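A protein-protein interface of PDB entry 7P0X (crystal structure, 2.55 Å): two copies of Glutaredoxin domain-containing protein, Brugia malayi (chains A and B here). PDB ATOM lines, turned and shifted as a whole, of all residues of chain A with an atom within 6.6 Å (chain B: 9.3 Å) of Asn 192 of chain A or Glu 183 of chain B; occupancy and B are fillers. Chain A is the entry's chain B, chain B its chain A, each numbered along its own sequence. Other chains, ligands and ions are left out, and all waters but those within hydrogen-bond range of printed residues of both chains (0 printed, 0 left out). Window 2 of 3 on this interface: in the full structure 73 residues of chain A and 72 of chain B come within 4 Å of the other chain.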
ATOM      1  N   ALA A 188      34.787  34.401  -9.583  1.00  0.00           N
ATOM      2  CA  ALA A 188      34.410  33.422  -8.526  1.00  0.00           C
ATOM      3  C   ALA A 188      32.890  33.223  -8.592  1.00  0.00           C
ATOM      4  O   ALA A 188      32.177  34.210  -8.891  1.00  0.00           O
ATOM      5  CB  ALA A 188      34.835  33.902  -7.160  1.00  0.00           C
ATOM      6  N   ILE A 189      32.418  31.998  -8.372  1.00  0.00           N
ATOM      7  CA  ILE A 189      30.979  31.625  -8.484  1.00  0.00           C
ATOM      8  C   ILE A 189      30.533  31.058  -7.140  1.00  0.00           C
ATOM      9  O   ILE A 189      31.121  30.079  -6.706  1.00  0.00           O
ATOM     10  CB  ILE A 189      30.761  30.611  -9.616  1.00  0.00           C
ATOM     11  CG1 ILE A 189      31.202  31.163 -10.972  1.00  0.00           C
ATOM     12  CG2 ILE A 189      29.308  30.168  -9.634  1.00  0.00           C
ATOM     13  CD1 ILE A 189      31.620  30.091 -11.950  1.00  0.00           C
ATOM     14  N   LYS A 190      29.548  31.683  -6.513  1.00  0.00           N
ATOM     15  CA  LYS A 190      29.058  31.352  -5.156  1.00  0.00           C
ATOM     16  C   LYS A 190      27.792  30.513  -5.314  1.00  0.00           C
ATOM     17  O   LYS A 190      27.080  30.699  -6.320  1.00  0.00           O
ATOM     18  CB  LYS A 190      28.765  32.620  -4.337  1.00  0.00           C
ATOM     19  CG  LYS A 190      29.932  33.192  -3.541  1.00  0.00           C
ATOM     20  CD  LYS A 190      29.750  34.666  -3.168  1.00  0.00           C
ATOM     21  CE  LYS A 190      28.554  34.944  -2.274  1.00  0.00           C
ATOM     22  NZ  LYS A 190      28.591  36.329  -1.743  1.00  0.00           N
ATOM     23  N   LEU A 191      27.541  29.636  -4.335  1.00  0.00           N
ATOM     24  CA  LEU A 191      26.257  28.906  -4.171  1.00  0.00           C
ATOM     25  C   LEU A 191      25.379  29.737  -3.233  1.00  0.00           C
ATOM     26  O   LEU A 191      25.799  29.983  -2.096  1.00  0.00           O
ATOM     27  CB  LEU A 191      26.560  27.518  -3.599  1.00  0.00           C
ATOM     28  CG  LEU A 191      25.392  26.543  -3.410  1.00  0.00           C
ATOM     29  CD1 LEU A 191      24.510  26.920  -2.232  1.00  0.00           C
ATOM     30  CD2 LEU A 191      24.571  26.371  -4.672  1.00  0.00           C
ATOM     31  N   ASN A 192      24.210  30.158  -3.711  1.00  0.00           N
ATOM     32  CA  ASN A 192      23.158  30.831  -2.911  1.00  0.00           C
ATOM     33  C   ASN A 192      22.376  29.777  -2.119  1.00  0.00           C
ATOM     34  O   ASN A 192      21.590  29.025  -2.720  1.00  0.00           O
ATOM     35  CB  ASN A 192      22.238  31.615  -3.835  1.00  0.00           C
ATOM     36  CG  ASN A 192      21.307  32.533  -3.080  1.00  0.00           C
ATOM     37  OD1 ASN A 192      20.637  32.119  -2.139  1.00  0.00           O
ATOM     38  ND2 ASN A 192      21.301  33.784  -3.481  1.00  0.00           N
ATOM     39  N   TRP A 193      22.565  29.732  -0.807  1.00  0.00           N
ATOM     40  CA  TRP A 193      21.945  28.712   0.077  1.00  0.00           C
ATOM     41  C   TRP A 193      20.416  28.759  -0.035  1.00  0.00           C
ATOM     42  O   TRP A 193      19.770  27.699  -0.082  1.00  0.00           O
ATOM     43  CB  TRP A 193      22.417  28.898   1.517  1.00  0.00           C
ATOM     44  CG  TRP A 193      21.681  28.006   2.463  1.00  0.00           C
ATOM     45  CD1 TRP A 193      20.534  28.300   3.141  1.00  0.00           C
ATOM     46  CD2 TRP A 193      21.998  26.645   2.791  1.00  0.00           C
ATOM     47  NE1 TRP A 193      20.133  27.228   3.887  1.00  0.00           N
ATOM     48  CE2 TRP A 193      21.012  26.197   3.693  1.00  0.00           C
ATOM     49  CE3 TRP A 193      23.021  25.766   2.432  1.00  0.00           C
ATOM     50  CZ2 TRP A 193      21.024  24.918   4.244  1.00  0.00           C
ATOM     51  CZ3 TRP A 193      23.026  24.491   2.969  1.00  0.00           C
ATOM     52  CH2 TRP A 193      22.041  24.079   3.867  1.00  0.00           C
ATOM     53  N   HIS A 194      19.840  29.946  -0.071  1.00  0.00           N
ATOM     54  CA  HIS A 194      18.368  30.172  -0.079  1.00  0.00           C
ATOM     55  C   HIS A 194      17.753  29.506  -1.320  1.00  0.00           C
ATOM     56  O   HIS A 194      16.724  28.802  -1.158  1.00  0.00           O
ATOM     57  CB  HIS A 194      18.068  31.671   0.106  1.00  0.00           C
ATOM     58  CG  HIS A 194      18.451  32.155   1.471  1.00  0.00           C
ATOM     59  ND1 HIS A 194      19.545  32.995   1.691  1.00  0.00           N
ATOM     60  CD2 HIS A 194      17.935  31.864   2.695  1.00  0.00           C
ATOM     61  CE1 HIS A 194      19.684  33.193   2.986  1.00  0.00           C
ATOM     62  NE2 HIS A 194      18.711  32.507   3.618  1.00  0.00           N
ATOM     63  N   GLN A 195      18.384  29.645  -2.491  1.00  0.00           N
ATOM     64  CA  GLN A 195      17.878  29.039  -3.754  1.00  0.00           C
ATOM     65  C   GLN A 195      17.929  27.508  -3.629  1.00  0.00           C
ATOM     66  O   GLN A 195      16.901  26.866  -3.951  1.00  0.00           O
ATOM     67  CB  GLN A 195      18.642  29.564  -4.972  1.00  0.00           C
ATOM     68  CG  GLN A 195      18.262  30.993  -5.352  1.00  0.00           C
ATOM     69  CD  GLN A 195      19.138  31.550  -6.461  1.00  0.00           C
ATOM     70  OE1 GLN A 195      19.807  30.809  -7.190  1.00  0.00           O
ATOM     71  NE2 GLN A 195      19.174  32.872  -6.583  1.00  0.00           N
ATOM     72  N   LEU A 196      19.050  26.950  -3.140  1.00  0.00           N
ATOM     73  CA  LEU A 196      19.246  25.489  -2.958  1.00  0.00           C
ATOM     74  C   LEU A 196      18.173  24.960  -2.009  1.00  0.00           C
ATOM     75  O   LEU A 196      17.413  23.998  -2.392  1.00  0.00           O
ATOM     76  CB  LEU A 196      20.647  25.193  -2.404  1.00  0.00           C
ATOM     77  CG  LEU A 196      20.960  23.713  -2.166  1.00  0.00           C
ATOM     78  CD1 LEU A 196      20.646  22.869  -3.402  1.00  0.00           C
ATOM     79  CD2 LEU A 196      22.424  23.509  -1.777  1.00  0.00           C
ATOM     80  N   LYS A 197      18.102  25.559  -0.822  1.00  0.00           N
ATOM     81  CA  LYS A 197      17.159  25.102   0.225  1.00  0.00           C
ATOM     82  C   LYS A 197      15.733  25.221  -0.301  1.00  0.00           C
ATOM     83  O   LYS A 197      14.961  24.286  -0.107  1.00  0.00           O
ATOM     84  CB  LYS A 197      17.362  25.938   1.485  1.00  0.00           C
ATOM     85  CG  LYS A 197      16.228  25.863   2.495  1.00  0.00           C
ATOM     86  CD  LYS A 197      15.958  27.183   3.170  1.00  0.00           C
ATOM     87  CE  LYS A 197      15.046  28.090   2.374  1.00  0.00           C
ATOM     88  NZ  LYS A 197      13.650  27.599   2.367  1.00  0.00           N
ATOM     89  N   ASN A 284      22.501  30.345   5.355  1.00  0.00           N
ATOM     90  CA  ASN A 284      23.758  29.631   5.033  1.00  0.00           C
ATOM     91  C   ASN A 284      24.428  29.296   6.362  1.00  0.00           C
ATOM     92  O   ASN A 284      24.649  30.198   7.185  1.00  0.00           O
ATOM     93  CB  ASN A 284      24.679  30.443   4.122  1.00  0.00           C
ATOM     94  CG  ASN A 284      25.800  29.589   3.579  1.00  0.00           C
ATOM     95  OD1 ASN A 284      26.408  28.827   4.319  1.00  0.00           O
ATOM     96  ND2 ASN A 284      26.043  29.661   2.284  1.00  0.00           N
ATOM     97  N   ILE B 174      25.879  22.806 -16.484  1.00  0.00           N
ATOM     98  CA  ILE B 174      25.946  24.275 -16.198  1.00  0.00           C
ATOM     99  C   ILE B 174      24.535  24.791 -15.900  1.00  0.00           C
ATOM    100  O   ILE B 174      24.391  25.603 -14.980  1.00  0.00           O
ATOM    101  CB  ILE B 174      26.635  25.071 -17.320  1.00  0.00           C
ATOM    102  CG1 ILE B 174      28.132  24.772 -17.367  1.00  0.00           C
ATOM    103  CG2 ILE B 174      26.390  26.565 -17.142  1.00  0.00           C
ATOM    104  CD1 ILE B 174      28.790  25.154 -18.666  1.00  0.00           C
ATOM    105  N   ASP B 176      21.833  23.104 -14.828  1.00  0.00           N
ATOM    106  CA  ASP B 176      21.431  22.496 -13.530  1.00  0.00           C
ATOM    107  C   ASP B 176      22.050  23.289 -12.378  1.00  0.00           C
ATOM    108  O   ASP B 176      21.300  23.630 -11.371  1.00  0.00           O
ATOM    109  CB  ASP B 176      21.882  21.039 -13.441  1.00  0.00           C
ATOM    110  CG  ASP B 176      21.205  20.094 -14.416  1.00  0.00           C
ATOM    111  OD1 ASP B 176      20.226  20.499 -15.045  1.00  0.00           O
ATOM    112  OD2 ASP B 176      21.647  18.961 -14.494  1.00  0.00           O
ATOM    113  N   ALA B 177      23.346  23.599 -12.522  1.00  0.00           N
ATOM    114  CA  ALA B 177      24.106  24.380 -11.512  1.00  0.00           C
ATOM    115  C   ALA B 177      23.327  25.648 -11.119  1.00  0.00           C
ATOM    116  O   ALA B 177      23.254  25.957  -9.890  1.00  0.00           O
ATOM    117  CB  ALA B 177      25.490  24.700 -12.008  1.00  0.00           C
ATOM    118  N   LYS B 178      22.717  26.340 -12.087  1.00  0.00           N
ATOM    119  CA  LYS B 178      21.957  27.595 -11.821  1.00  0.00           C
ATOM    120  C   LYS B 178      20.726  27.260 -10.978  1.00  0.00           C
ATOM    121  O   LYS B 178      20.426  28.026 -10.034  1.00  0.00           O
ATOM    122  CB  LYS B 178      21.507  28.296 -13.102  1.00  0.00           C
ATOM    123  CG  LYS B 178      22.640  28.760 -14.005  1.00  0.00           C
ATOM    124  CD  LYS B 178      22.156  29.407 -15.268  1.00  0.00           C
ATOM    125  CE  LYS B 178      23.290  29.794 -16.191  1.00  0.00           C
ATOM    126  NZ  LYS B 178      22.771  30.492 -17.388  1.00  0.00           N
ATOM    127  N   LYS B 179      20.064  26.146 -11.285  1.00  0.00           N
ATOM    128  CA  LYS B 179      18.793  25.752 -10.629  1.00  0.00           C
ATOM    129  C   LYS B 179      19.101  25.213  -9.231  1.00  0.00           C
ATOM    130  O   LYS B 179      18.197  25.258  -8.406  1.00  0.00           O
ATOM    131  CB  LYS B 179      18.054  24.695 -11.458  1.00  0.00           C
ATOM    132  CG  LYS B 179      17.782  25.081 -12.910  1.00  0.00           C
ATOM    133  CD  LYS B 179      16.630  26.047 -13.090  1.00  0.00           C
ATOM    134  CE  LYS B 179      15.297  25.369 -12.867  1.00  0.00           C
ATOM    135  NZ  LYS B 179      14.184  26.341 -12.809  1.00  0.00           N
ATOM    136  N   PHE B 180      20.315  24.711  -8.969  1.00  0.00           N
ATOM    137  CA  PHE B 180      20.690  24.302  -7.585  1.00  0.00           C
ATOM    138  C   PHE B 180      21.255  25.492  -6.793  1.00  0.00           C
ATOM    139  O   PHE B 180      21.623  25.286  -5.614  1.00  0.00           O
ATOM    140  CB  PHE B 180      21.684  23.148  -7.594  1.00  0.00           C
ATOM    141  CG  PHE B 180      21.074  21.799  -7.844  1.00  0.00           C
ATOM    142  CD1 PHE B 180      20.821  21.383  -9.140  1.00  0.00           C
ATOM    143  CD2 PHE B 180      20.807  20.936  -6.805  1.00  0.00           C
ATOM    144  CE1 PHE B 180      20.293  20.124  -9.389  1.00  0.00           C
ATOM    145  CE2 PHE B 180      20.285  19.677  -7.050  1.00  0.00           C
ATOM    146  CZ  PHE B 180      20.039  19.257  -8.339  1.00  0.00           C
ATOM    147  N   GLY B 181      21.406  26.659  -7.430  1.00  0.00           N
ATOM    148  CA  GLY B 181      21.725  27.936  -6.765  1.00  0.00           C
ATOM    149  C   GLY B 181      23.131  28.463  -7.041  1.00  0.00           C
ATOM    150  O   GLY B 181      23.564  29.395  -6.373  1.00  0.00           O
ATOM    151  N   TRP B 182      23.885  27.869  -7.942  1.00  0.00           N
ATOM    152  CA  TRP B 182      25.215  28.428  -8.293  1.00  0.00           C
ATOM    153  C   TRP B 182      24.987  29.718  -9.088  1.00  0.00           C
ATOM    154  O   TRP B 182      24.244  29.661 -10.075  1.00  0.00           O
ATOM    155  CB  TRP B 182      26.074  27.403  -9.047  1.00  0.00           C
ATOM    156  CG  TRP B 182      26.555  26.307  -8.151  1.00  0.00           C
ATOM    157  CD1 TRP B 182      25.982  25.078  -7.983  1.00  0.00           C
ATOM    158  CD2 TRP B 182      27.699  26.346  -7.283  1.00  0.00           C
ATOM    159  NE1 TRP B 182      26.683  24.363  -7.050  1.00  0.00           N
ATOM    160  CE2 TRP B 182      27.751  25.098  -6.617  1.00  0.00           C
ATOM    161  CE3 TRP B 182      28.683  27.296  -7.002  1.00  0.00           C
ATOM    162  CZ2 TRP B 182      28.738  24.787  -5.684  1.00  0.00           C
ATOM    163  CZ3 TRP B 182      29.674  26.978  -6.096  1.00  0.00           C
ATOM    164  CH2 TRP B 182      29.698  25.743  -5.440  1.00  0.00           C
ATOM    165  N   GLU B 183      25.552  30.842  -8.644  1.00  0.00           N
ATOM    166  CA  GLU B 183      25.372  32.162  -9.321  1.00  0.00           C
ATOM    167  C   GLU B 183      26.413  32.240 -10.439  1.00  0.00           C
ATOM    168  O   GLU B 183      27.535  32.706 -10.190  1.00  0.00           O
ATOM    169  CB  GLU B 183      25.400  33.306  -8.311  1.00  0.00           C
ATOM    170  CG  GLU B 183      24.225  33.228  -7.347  1.00  0.00           C
ATOM    171  CD  GLU B 183      24.370  34.134  -6.054  1.00  0.00           C
ATOM    172  OE1 GLU B 183      25.535  34.513  -5.730  1.00  0.00           O
ATOM    173  OE2 GLU B 183      23.333  34.450  -5.398  1.00  0.00           O
ATOM    174  N   ILE B 184      26.040  31.724 -11.610  1.00  0.00           N
ATOM    175  CA  ILE B 184      26.830  31.777 -12.867  1.00  0.00           C
ATOM    176  C   ILE B 184      26.519  33.107 -13.543  1.00  0.00           C
ATOM    177  O   ILE B 184      25.348  33.355 -13.854  1.00  0.00           O
ATOM    178  CB  ILE B 184      26.423  30.606 -13.777  1.00  0.00           C
ATOM    179  CG1 ILE B 184      26.494  29.256 -13.059  1.00  0.00           C
ATOM    180  CG2 ILE B 184      27.220  30.633 -15.072  1.00  0.00           C
ATOM    181  CD1 ILE B 184      27.812  28.560 -13.176  1.00  0.00           C
ATOM    182  N   PRO B 185      27.512  34.002 -13.792  1.00  0.00           N
ATOM    183  CA  PRO B 185      27.246  35.229 -14.546  1.00  0.00           C
ATOM    184  C   PRO B 185      26.345  34.956 -15.763  1.00  0.00           C
ATOM    185  O   PRO B 185      26.438  33.876 -16.365  1.00  0.00           O
ATOM    186  CB  PRO B 185      28.654  35.734 -14.889  1.00  0.00           C
ATOM    187  CG  PRO B 185      29.492  35.279 -13.702  1.00  0.00           C
ATOM    188  CD  PRO B 185      28.908  33.926 -13.322  1.00  0.00           C
ATOM    189  N   GLU B 186      25.445  35.914 -16.058  1.00  0.00           N
ATOM    190  CA  GLU B 186      24.288  35.720 -16.977  1.00  0.00           C
ATOM    191  C   GLU B 186      24.794  35.934 -18.406  1.00  0.00           C
ATOM    192  O   GLU B 186      25.872  36.566 -18.562  1.00  0.00           O
ATOM    193  CB  GLU B 186      23.073  36.558 -16.545  1.00  0.00           C
ATOM    194  CG  GLU B 186      22.039  35.707 -15.811  1.00  0.00           C
ATOM    195  CD  GLU B 186      21.714  34.382 -16.508  1.00  0.00           C
ATOM    196  OE1 GLU B 186      21.605  34.397 -17.761  1.00  0.00           O
ATOM    197  OE2 GLU B 186      21.618  33.317 -15.823  1.00  0.00           O
ATOM    198  N   ILE B 189      26.900  31.082 -23.025  1.00  0.00           N
ATOM    199  CA  ILE B 189      28.220  30.445 -22.763  1.00  0.00           C
ATOM    200  C   ILE B 189      28.528  29.531 -23.945  1.00  0.00           C
ATOM    201  O   ILE B 189      27.711  28.640 -24.201  1.00  0.00           O
ATOM    202  CB  ILE B 189      28.201  29.676 -21.438  1.00  0.00           C
ATOM    203  CG1 ILE B 189      27.948  30.611 -20.249  1.00  0.00           C
ATOM    204  CG2 ILE B 189      29.492  28.876 -21.288  1.00  0.00           C
ATOM    205  CD1 ILE B 189      27.267  29.942 -19.079  1.00  0.00           C
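The backbone carbonyl oxygen (O) of Gly 181 of chain B is in hydrogen-bond range of the backbone NH (N) of Asn 192 of chain A, at 2.8 Å. The backbone NH (N) of Glu 183 of chain B lies within hydrogen-bond range of the backbone carbonyl oxygen (O) of Lys 190 of chain A (2.8 Å). The side-chain amide nitrogen of Asn 192 of chain A sits at hydrogen-bond distance from the side-chain carboxylate of Glu 183 of chain B (2.9 Å).
The backbone NH (N) of Trp 182 of chain B sits at hydrogen-bond distance from the backbone carbonyl oxygen (O) of Ala 177 of chain B. The backbone NH (N) of His 194 of chain A is in hydrogen-bond range of the side-chain amide oxygen (OD1) of Asn 192 of chain A, 3.1 Å away. The backbone NH of Gln 195 of chain A lies within hydrogen-bond range of the side-chain amide oxygen of Asn 192 of chain A, at 3.4 Å.
Among the printed residues, pairs that only touch across the chains: Ile 189 of chain A with Trp 182 of chain B, Ile 189 of chain A with Glu 183 of chain B, Lys 190 of chain A with Gly 181 of chain B, Lys 190 of chain A with Trp 182 of chain B, Leu 191 of chain A with Phe 180 of chain B, Leu 191 of chain A with Gly 181 of chain B, Leu 191 of chain A with Trp 182 of chain B, Gln 195 of chain A with Gly 181 of chain B and Leu 196 of chain A with Phe 180 of chain B.
Asn 192 of chain A touches two residues of chain B. Of chain A, only Ile 189, Lys 190 and Asn 192 come within 4 Å of Glu 183 of chain B. Of the printed residues of chain B, Leu 196 of chain A touches Phe 180 (3.4 Å). Of the printed residues of chain B, Gln 195 of chain A touches Gly 181. Of the printed residues of chain A, Trp 182 of chain B touches Ile 189, Lys 190 and Leu 191. Printed residues of chain A within 4 Å of Gly 181 of chain B: Lys 190, Leu 191, Asn 192 and Gln 195. The nearest residue of chain B that does not touch Asn 192 of chain A is Phe 180 of chain B (4.7 Å). The nearest residue of chain A that does not touch Glu 183 of chain B is Gln 195 of chain A (4.6 Å). The nearest printed residue of chain B that does not touch Ile 189 of chain A is Ile 184 of chain B (4.1 Å).
Of the 13 printed residues of chain B, 4 touch a printed residue of chain A. Hydrophobic or aromatic side chains of chain A that line the printed part of chain B: Ile 189, Leu 191 and Leu 196. Among the printed residues, 12 pairs touch across the chains. Among the printed residues, no Asp or Glu carboxylate lies within 4 Å of a Lys or Arg side-chain nitrogen of the other chain.
Position printed for both chains: 189. Of the 12 pairs that touch across the chains among the printed residues, none has its exchanged pair printed and touching as well.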
